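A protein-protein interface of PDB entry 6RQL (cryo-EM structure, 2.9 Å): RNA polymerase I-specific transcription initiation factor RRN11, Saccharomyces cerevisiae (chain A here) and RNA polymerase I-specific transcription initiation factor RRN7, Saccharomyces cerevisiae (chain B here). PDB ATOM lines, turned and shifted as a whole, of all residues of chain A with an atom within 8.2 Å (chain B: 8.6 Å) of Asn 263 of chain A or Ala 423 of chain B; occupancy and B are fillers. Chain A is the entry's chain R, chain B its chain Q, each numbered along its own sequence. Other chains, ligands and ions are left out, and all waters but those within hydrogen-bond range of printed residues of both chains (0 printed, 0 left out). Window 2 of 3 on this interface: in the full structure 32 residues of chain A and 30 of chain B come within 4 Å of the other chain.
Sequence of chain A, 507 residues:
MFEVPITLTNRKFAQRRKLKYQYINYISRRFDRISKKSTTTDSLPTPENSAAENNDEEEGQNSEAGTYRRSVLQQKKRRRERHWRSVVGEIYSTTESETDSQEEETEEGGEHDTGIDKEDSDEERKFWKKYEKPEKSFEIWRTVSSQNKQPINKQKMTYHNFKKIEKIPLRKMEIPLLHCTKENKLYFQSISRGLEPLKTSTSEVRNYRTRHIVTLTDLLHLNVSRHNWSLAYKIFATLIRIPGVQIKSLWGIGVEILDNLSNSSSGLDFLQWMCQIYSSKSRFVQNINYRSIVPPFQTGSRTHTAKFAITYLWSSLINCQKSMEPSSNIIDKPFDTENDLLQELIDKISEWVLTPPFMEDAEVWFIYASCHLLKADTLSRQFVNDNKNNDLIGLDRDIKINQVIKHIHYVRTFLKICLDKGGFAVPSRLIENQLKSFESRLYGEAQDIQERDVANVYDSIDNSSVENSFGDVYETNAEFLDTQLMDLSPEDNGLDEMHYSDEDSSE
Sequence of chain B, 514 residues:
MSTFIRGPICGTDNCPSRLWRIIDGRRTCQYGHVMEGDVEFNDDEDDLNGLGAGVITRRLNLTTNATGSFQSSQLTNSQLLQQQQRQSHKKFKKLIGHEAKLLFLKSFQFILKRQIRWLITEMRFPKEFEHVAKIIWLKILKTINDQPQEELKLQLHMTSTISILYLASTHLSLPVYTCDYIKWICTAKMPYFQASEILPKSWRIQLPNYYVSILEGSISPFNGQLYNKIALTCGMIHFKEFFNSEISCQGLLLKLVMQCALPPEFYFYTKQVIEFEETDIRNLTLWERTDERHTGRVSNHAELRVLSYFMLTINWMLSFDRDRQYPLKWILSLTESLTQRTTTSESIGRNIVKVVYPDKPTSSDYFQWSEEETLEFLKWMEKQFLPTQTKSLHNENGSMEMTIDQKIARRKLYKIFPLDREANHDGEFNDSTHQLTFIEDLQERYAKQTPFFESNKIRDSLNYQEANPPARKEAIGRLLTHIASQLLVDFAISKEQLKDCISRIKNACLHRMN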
ATOM      1  N   TYR A 233      32.772  23.920  18.592  1.00  0.00           N
ATOM      2  CA  TYR A 233      31.733  22.901  18.882  1.00  0.00           C
ATOM      3  C   TYR A 233      31.565  21.974  17.675  1.00  0.00           C
ATOM      4  O   TYR A 233      31.410  20.769  17.864  1.00  0.00           O
ATOM      5  CB  TYR A 233      30.391  23.534  19.234  1.00  0.00           C
ATOM      6  CG  TYR A 233      29.286  22.517  19.312  1.00  0.00           C
ATOM      7  CD1 TYR A 233      28.862  22.001  20.520  1.00  0.00           C
ATOM      8  CD2 TYR A 233      28.697  22.036  18.159  1.00  0.00           C
ATOM      9  CE1 TYR A 233      27.865  21.046  20.582  1.00  0.00           C
ATOM     10  CE2 TYR A 233      27.698  21.083  18.202  1.00  0.00           C
ATOM     11  CZ  TYR A 233      27.281  20.587  19.417  1.00  0.00           C
ATOM     12  OH  TYR A 233      26.291  19.653  19.447  1.00  0.00           O
ATOM     13  N   ILE A 257      30.198  24.215  25.507  1.00  0.00           N
ATOM     14  CA  ILE A 257      28.805  24.383  25.903  1.00  0.00           C
ATOM     15  C   ILE A 257      28.698  25.390  27.034  1.00  0.00           C
ATOM     16  O   ILE A 257      27.745  26.175  27.094  1.00  0.00           O
ATOM     17  CB  ILE A 257      28.219  23.023  26.307  1.00  0.00           C
ATOM     18  CG1 ILE A 257      28.310  22.031  25.160  1.00  0.00           C
ATOM     19  CG2 ILE A 257      26.770  23.143  26.684  1.00  0.00           C
ATOM     20  CD1 ILE A 257      27.900  20.658  25.574  1.00  0.00           C
ATOM     21  N   ASN A 260      29.133  28.627  25.089  1.00  0.00           N
ATOM     22  CA  ASN A 260      28.199  28.883  23.999  1.00  0.00           C
ATOM     23  C   ASN A 260      26.994  29.664  24.504  1.00  0.00           C
ATOM     24  O   ASN A 260      26.736  30.789  24.064  1.00  0.00           O
ATOM     25  CB  ASN A 260      27.751  27.556  23.385  1.00  0.00           C
ATOM     26  CG  ASN A 260      27.110  27.713  22.039  1.00  0.00           C
ATOM     27  OD1 ASN A 260      27.007  28.813  21.506  1.00  0.00           O
ATOM     28  ND2 ASN A 260      26.666  26.600  21.472  1.00  0.00           N
ATOM     29  N   LEU A 261      26.228  29.052  25.411  1.00  0.00           N
ATOM     30  CA  LEU A 261      25.160  29.661  26.206  1.00  0.00           C
ATOM     31  C   LEU A 261      24.002  30.195  25.369  1.00  0.00           C
ATOM     32  O   LEU A 261      23.199  30.993  25.864  1.00  0.00           O
ATOM     33  CB  LEU A 261      25.705  30.772  27.109  1.00  0.00           C
ATOM     34  CG  LEU A 261      26.728  30.304  28.145  1.00  0.00           C
ATOM     35  CD1 LEU A 261      27.334  31.483  28.893  1.00  0.00           C
ATOM     36  CD2 LEU A 261      26.116  29.304  29.114  1.00  0.00           C
ATOM     37  N   SER A 262      23.889  29.787  24.107  1.00  0.00           N
ATOM     38  CA  SER A 262      22.753  30.161  23.278  1.00  0.00           C
ATOM     39  C   SER A 262      21.811  28.990  23.042  1.00  0.00           C
ATOM     40  O   SER A 262      20.621  29.074  23.358  1.00  0.00           O
ATOM     41  CB  SER A 262      23.244  30.722  21.940  1.00  0.00           C
ATOM     42  OG  SER A 262      22.155  31.104  21.123  1.00  0.00           O
ATOM     43  N   ASN A 263      22.333  27.893  22.509  1.00  0.00           N
ATOM     44  CA  ASN A 263      21.613  26.640  22.310  1.00  0.00           C
ATOM     45  C   ASN A 263      22.198  25.587  23.224  1.00  0.00           C
ATOM     46  O   ASN A 263      22.427  24.436  22.850  1.00  0.00           O
ATOM     47  CB  ASN A 263      21.686  26.212  20.854  1.00  0.00           C
ATOM     48  CG  ASN A 263      20.824  27.070  19.963  1.00  0.00           C
ATOM     49  OD1 ASN A 263      19.651  27.295  20.250  1.00  0.00           O
ATOM     50  ND2 ASN A 263      21.413  27.597  18.898  1.00  0.00           N
ATOM     51  N   SER A 264      22.445  26.009  24.459  1.00  0.00           N
ATOM     52  CA  SER A 264      23.312  25.288  25.373  1.00  0.00           C
ATOM     53  C   SER A 264      22.651  24.029  25.914  1.00  0.00           C
ATOM     54  O   SER A 264      21.444  23.982  26.164  1.00  0.00           O
ATOM     55  CB  SER A 264      23.705  26.201  26.535  1.00  0.00           C
ATOM     56  OG  SER A 264      24.575  25.544  27.435  1.00  0.00           O
ATOM     57  N   SER A 265      23.470  22.994  26.087  1.00  0.00           N
ATOM     58  CA  SER A 265      23.147  21.860  26.941  1.00  0.00           C
ATOM     59  C   SER A 265      23.719  22.025  28.341  1.00  0.00           C
ATOM     60  O   SER A 265      24.125  21.036  28.967  1.00  0.00           O
ATOM     61  CB  SER A 265      23.636  20.568  26.302  1.00  0.00           C
ATOM     62  OG  SER A 265      22.953  20.317  25.089  1.00  0.00           O
ATOM     63  N   SER A 266      23.857  23.278  28.780  1.00  0.00           N
ATOM     64  CA  SER A 266      24.064  23.746  30.148  1.00  0.00           C
ATOM     65  C   SER A 266      25.468  23.496  30.688  1.00  0.00           C
ATOM     66  O   SER A 266      25.847  24.076  31.710  1.00  0.00           O
ATOM     67  CB  SER A 266      23.016  23.115  31.078  1.00  0.00           C
ATOM     68  OG  SER A 266      23.170  23.550  32.414  1.00  0.00           O
ATOM     69  N   LYS B 415      23.120  12.754  21.692  1.00  0.00           N
ATOM     70  CA  LYS B 415      21.976  13.615  21.952  1.00  0.00           C
ATOM     71  C   LYS B 415      22.399  14.932  22.586  1.00  0.00           C
ATOM     72  O   LYS B 415      21.790  15.969  22.313  1.00  0.00           O
ATOM     73  CB  LYS B 415      20.980  12.888  22.855  1.00  0.00           C
ATOM     74  CG  LYS B 415      19.694  13.638  23.112  1.00  0.00           C
ATOM     75  CD  LYS B 415      18.870  13.734  21.845  1.00  0.00           C
ATOM     76  CE  LYS B 415      17.564  14.456  22.097  1.00  0.00           C
ATOM     77  NZ  LYS B 415      16.783  14.657  20.846  1.00  0.00           N
ATOM     78  N   ILE B 416      23.440  14.921  23.415  1.00  0.00           N
ATOM     79  CA  ILE B 416      23.907  16.173  23.997  1.00  0.00           C
ATOM     80  C   ILE B 416      24.815  16.926  23.033  1.00  0.00           C
ATOM     81  O   ILE B 416      24.888  18.159  23.091  1.00  0.00           O
ATOM     82  CB  ILE B 416      24.563  15.893  25.362  1.00  0.00           C
ATOM     83  CG1 ILE B 416      24.854  17.176  26.112  1.00  0.00           C
ATOM     84  CG2 ILE B 416      25.831  15.154  25.241  1.00  0.00           C
ATOM     85  CD1 ILE B 416      25.240  16.946  27.502  1.00  0.00           C
ATOM     86  N   PRO B 418      24.497  17.174  19.279  1.00  0.00           N
ATOM     87  CA  PRO B 418      23.913  16.879  17.973  1.00  0.00           C
ATOM     88  C   PRO B 418      24.841  17.347  16.870  1.00  0.00           C
ATOM     89  O   PRO B 418      25.552  18.345  17.017  1.00  0.00           O
ATOM     90  CB  PRO B 418      22.600  17.663  17.988  1.00  0.00           C
ATOM     91  CG  PRO B 418      22.852  18.765  18.920  1.00  0.00           C
ATOM     92  CD  PRO B 418      23.743  18.223  19.976  1.00  0.00           C
ATOM     93  N   ASP B 420      24.290  18.503  13.896  1.00  0.00           N
ATOM     94  CA  ASP B 420      23.888  19.650  13.101  1.00  0.00           C
ATOM     95  C   ASP B 420      24.440  20.944  13.687  1.00  0.00           C
ATOM     96  O   ASP B 420      24.984  20.976  14.797  1.00  0.00           O
ATOM     97  CB  ASP B 420      22.364  19.725  13.007  1.00  0.00           C
ATOM     98  CG  ASP B 420      21.679  19.830  14.374  1.00  0.00           C
ATOM     99  OD1 ASP B 420      22.336  19.702  15.423  1.00  0.00           O
ATOM    100  OD2 ASP B 420      20.456  20.059  14.402  1.00  0.00           O
ATOM    101  N   ARG B 421      24.292  22.032  12.939  1.00  0.00           N
ATOM    102  CA  ARG B 421      24.271  23.318  13.606  1.00  0.00           C
ATOM    103  C   ARG B 421      23.049  23.350  14.512  1.00  0.00           C
ATOM    104  O   ARG B 421      21.950  22.937  14.129  1.00  0.00           O
ATOM    105  CB  ARG B 421      24.247  24.478  12.610  1.00  0.00           C
ATOM    106  CG  ARG B 421      24.269  25.838  13.300  1.00  0.00           C
ATOM    107  CD  ARG B 421      24.267  27.008  12.340  1.00  0.00           C
ATOM    108  NE  ARG B 421      24.015  28.253  13.065  1.00  0.00           N
ATOM    109  CZ  ARG B 421      23.897  29.444  12.491  1.00  0.00           C
ATOM    110  NH1 ARG B 421      23.662  30.523  13.230  1.00  0.00           N
ATOM    111  NH2 ARG B 421      24.011  29.555  11.174  1.00  0.00           N
ATOM    112  N   GLU B 422      23.279  23.807  15.739  1.00  0.00           N
ATOM    113  CA  GLU B 422      22.302  23.733  16.816  1.00  0.00           C
ATOM    114  C   GLU B 422      21.026  24.524  16.525  1.00  0.00           C
ATOM    115  O   GLU B 422      19.955  24.147  17.014  1.00  0.00           O
ATOM    116  CB  GLU B 422      23.015  24.185  18.083  1.00  0.00           C
ATOM    117  CG  GLU B 422      23.759  25.488  17.863  1.00  0.00           C
ATOM    118  CD  GLU B 422      24.777  25.775  18.936  1.00  0.00           C
ATOM    119  OE1 GLU B 422      24.957  24.924  19.827  1.00  0.00           O
ATOM    120  OE2 GLU B 422      25.408  26.854  18.873  1.00  0.00           O
ATOM    121  N   ALA B 423      21.108  25.578  15.709  1.00  0.00           N
ATOM    122  CA  ALA B 423      19.927  26.271  15.199  1.00  0.00           C
ATOM    123  C   ALA B 423      20.304  27.052  13.950  1.00  0.00           C
ATOM    124  O   ALA B 423      21.437  27.517  13.817  1.00  0.00           O
ATOM    125  CB  ALA B 423      19.321  27.225  16.235  1.00  0.00           C
ATOM    126  N   ASN B 424      19.318  27.209  13.053  1.00  0.00           N
ATOM    127  CA  ASN B 424      19.371  28.076  11.865  1.00  0.00           C
ATOM    128  C   ASN B 424      20.502  27.668  10.912  1.00  0.00           C
ATOM    129  O   ASN B 424      21.467  28.397  10.676  1.00  0.00           O
ATOM    130  CB  ASN B 424      19.480  29.550  12.275  1.00  0.00           C
ATOM    131  CG  ASN B 424      18.200  30.073  12.884  1.00  0.00           C
ATOM    132  OD1 ASN B 424      17.112  29.837  12.360  1.00  0.00           O
ATOM    133  ND2 ASN B 424      18.317  30.759  14.012  1.00  0.00           N
ATOM    134  N   HIS B 425      20.327  26.475  10.350  1.00  0.00           N
ATOM    135  CA  HIS B 425      21.323  25.776   9.551  1.00  0.00           C
ATOM    136  C   HIS B 425      21.548  26.444   8.189  1.00  0.00           C
ATOM    137  O   HIS B 425      21.002  27.506   7.876  1.00  0.00           O
ATOM    138  CB  HIS B 425      20.902  24.320   9.366  1.00  0.00           C
ATOM    139  CG  HIS B 425      19.524  24.167   8.803  1.00  0.00           C
ATOM    140  ND1 HIS B 425      19.265  24.189   7.449  1.00  0.00           N
ATOM    141  CD2 HIS B 425      18.325  24.009   9.414  1.00  0.00           C
ATOM    142  CE1 HIS B 425      17.968  24.045   7.251  1.00  0.00           C
ATOM    143  NE2 HIS B 425      17.375  23.933   8.426  1.00  0.00           N
ATOM    144  N   ASP B 426      22.388  25.795   7.376  1.00  0.00           N
ATOM    145  CA  ASP B 426      22.812  26.310   6.079  1.00  0.00           C
ATOM    146  C   ASP B 426      22.294  25.485   4.902  1.00  0.00           C
ATOM    147  O   ASP B 426      22.984  25.380   3.879  1.00  0.00           O
ATOM    148  CB  ASP B 426      24.340  26.404   6.030  1.00  0.00           C
ATOM    149  CG  ASP B 426      25.032  25.079   6.332  1.00  0.00           C
ATOM    150  OD1 ASP B 426      24.357  24.106   6.728  1.00  0.00           O
ATOM    151  OD2 ASP B 426      26.265  25.005   6.160  1.00  0.00           O
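Of the printed residues of chain B, Tyr 233 of chain A touches Pro 418. Of the printed residues of chain B, Asn 260 of chain A touches Glu 422. No residue of chain B comes within 4 Å of Ser 262 of chain A. Asn 263 of chain A touches two residues of chain B. Printed residues of chain B within 4 Å of Ser 265 of chain A: Ile 416. Of the printed residues of chain A, Ile 416 of chain B touches Ser 265 (3.5 Å). Printed residues of chain A within 4 Å of Pro 418 of chain B: Tyr 233. Of chain A, only Asn 260 (2.9 Å) and Asn 263 (3.3 Å) come within 4 Å of Glu 422 of chain B. Ala 423 of chain B touches one residue of chain A. The nearest residue of chain B that does not touch Asn 263 of chain A is Asn 424 of chain B (6.2 Å).
The backbone carbonyl oxygen of Pro 418 of chain B lies within hydrogen-bond range of the side-chain hydroxyl of Tyr 233 of chain A. OE2 of Glu 422 of chain B lies within hydrogen-bond range of ND2 of Asn 260 of chain A (2.9 Å).
NE of Arg 421 of chain B lies within hydrogen-bond range of O of Ala 423 of chain B.
Among the printed residues, pairs that only touch across the chains: Asn 263 of chain A with Glu 422 of chain B (3.3 Å), Asn 263 of chain A with Ala 423 of chain B (3.4 Å) and Ser 265 of chain A with Ile 416 of chain B (3.5 Å).
Of the 10 printed residues of chain B, 4 touch a printed residue of chain A. Printed residues of chain B that touch a printed residue of chain A: Ile 416, Pro 418, Glu 422 and Ala 423. Hydrophobic or aromatic side chains of chain B that line the printed part of chain A: Ile 416, Pro 418 and Ala 423. Along chain B the printed residues that touch a printed residue of chain A span positions 416 to 423. Of the 9 printed residues of chain A, 4 touch a printed residue of chain B. Hydrophobic or aromatic side chains of chain A that line the printed part of chain B: Tyr 233.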
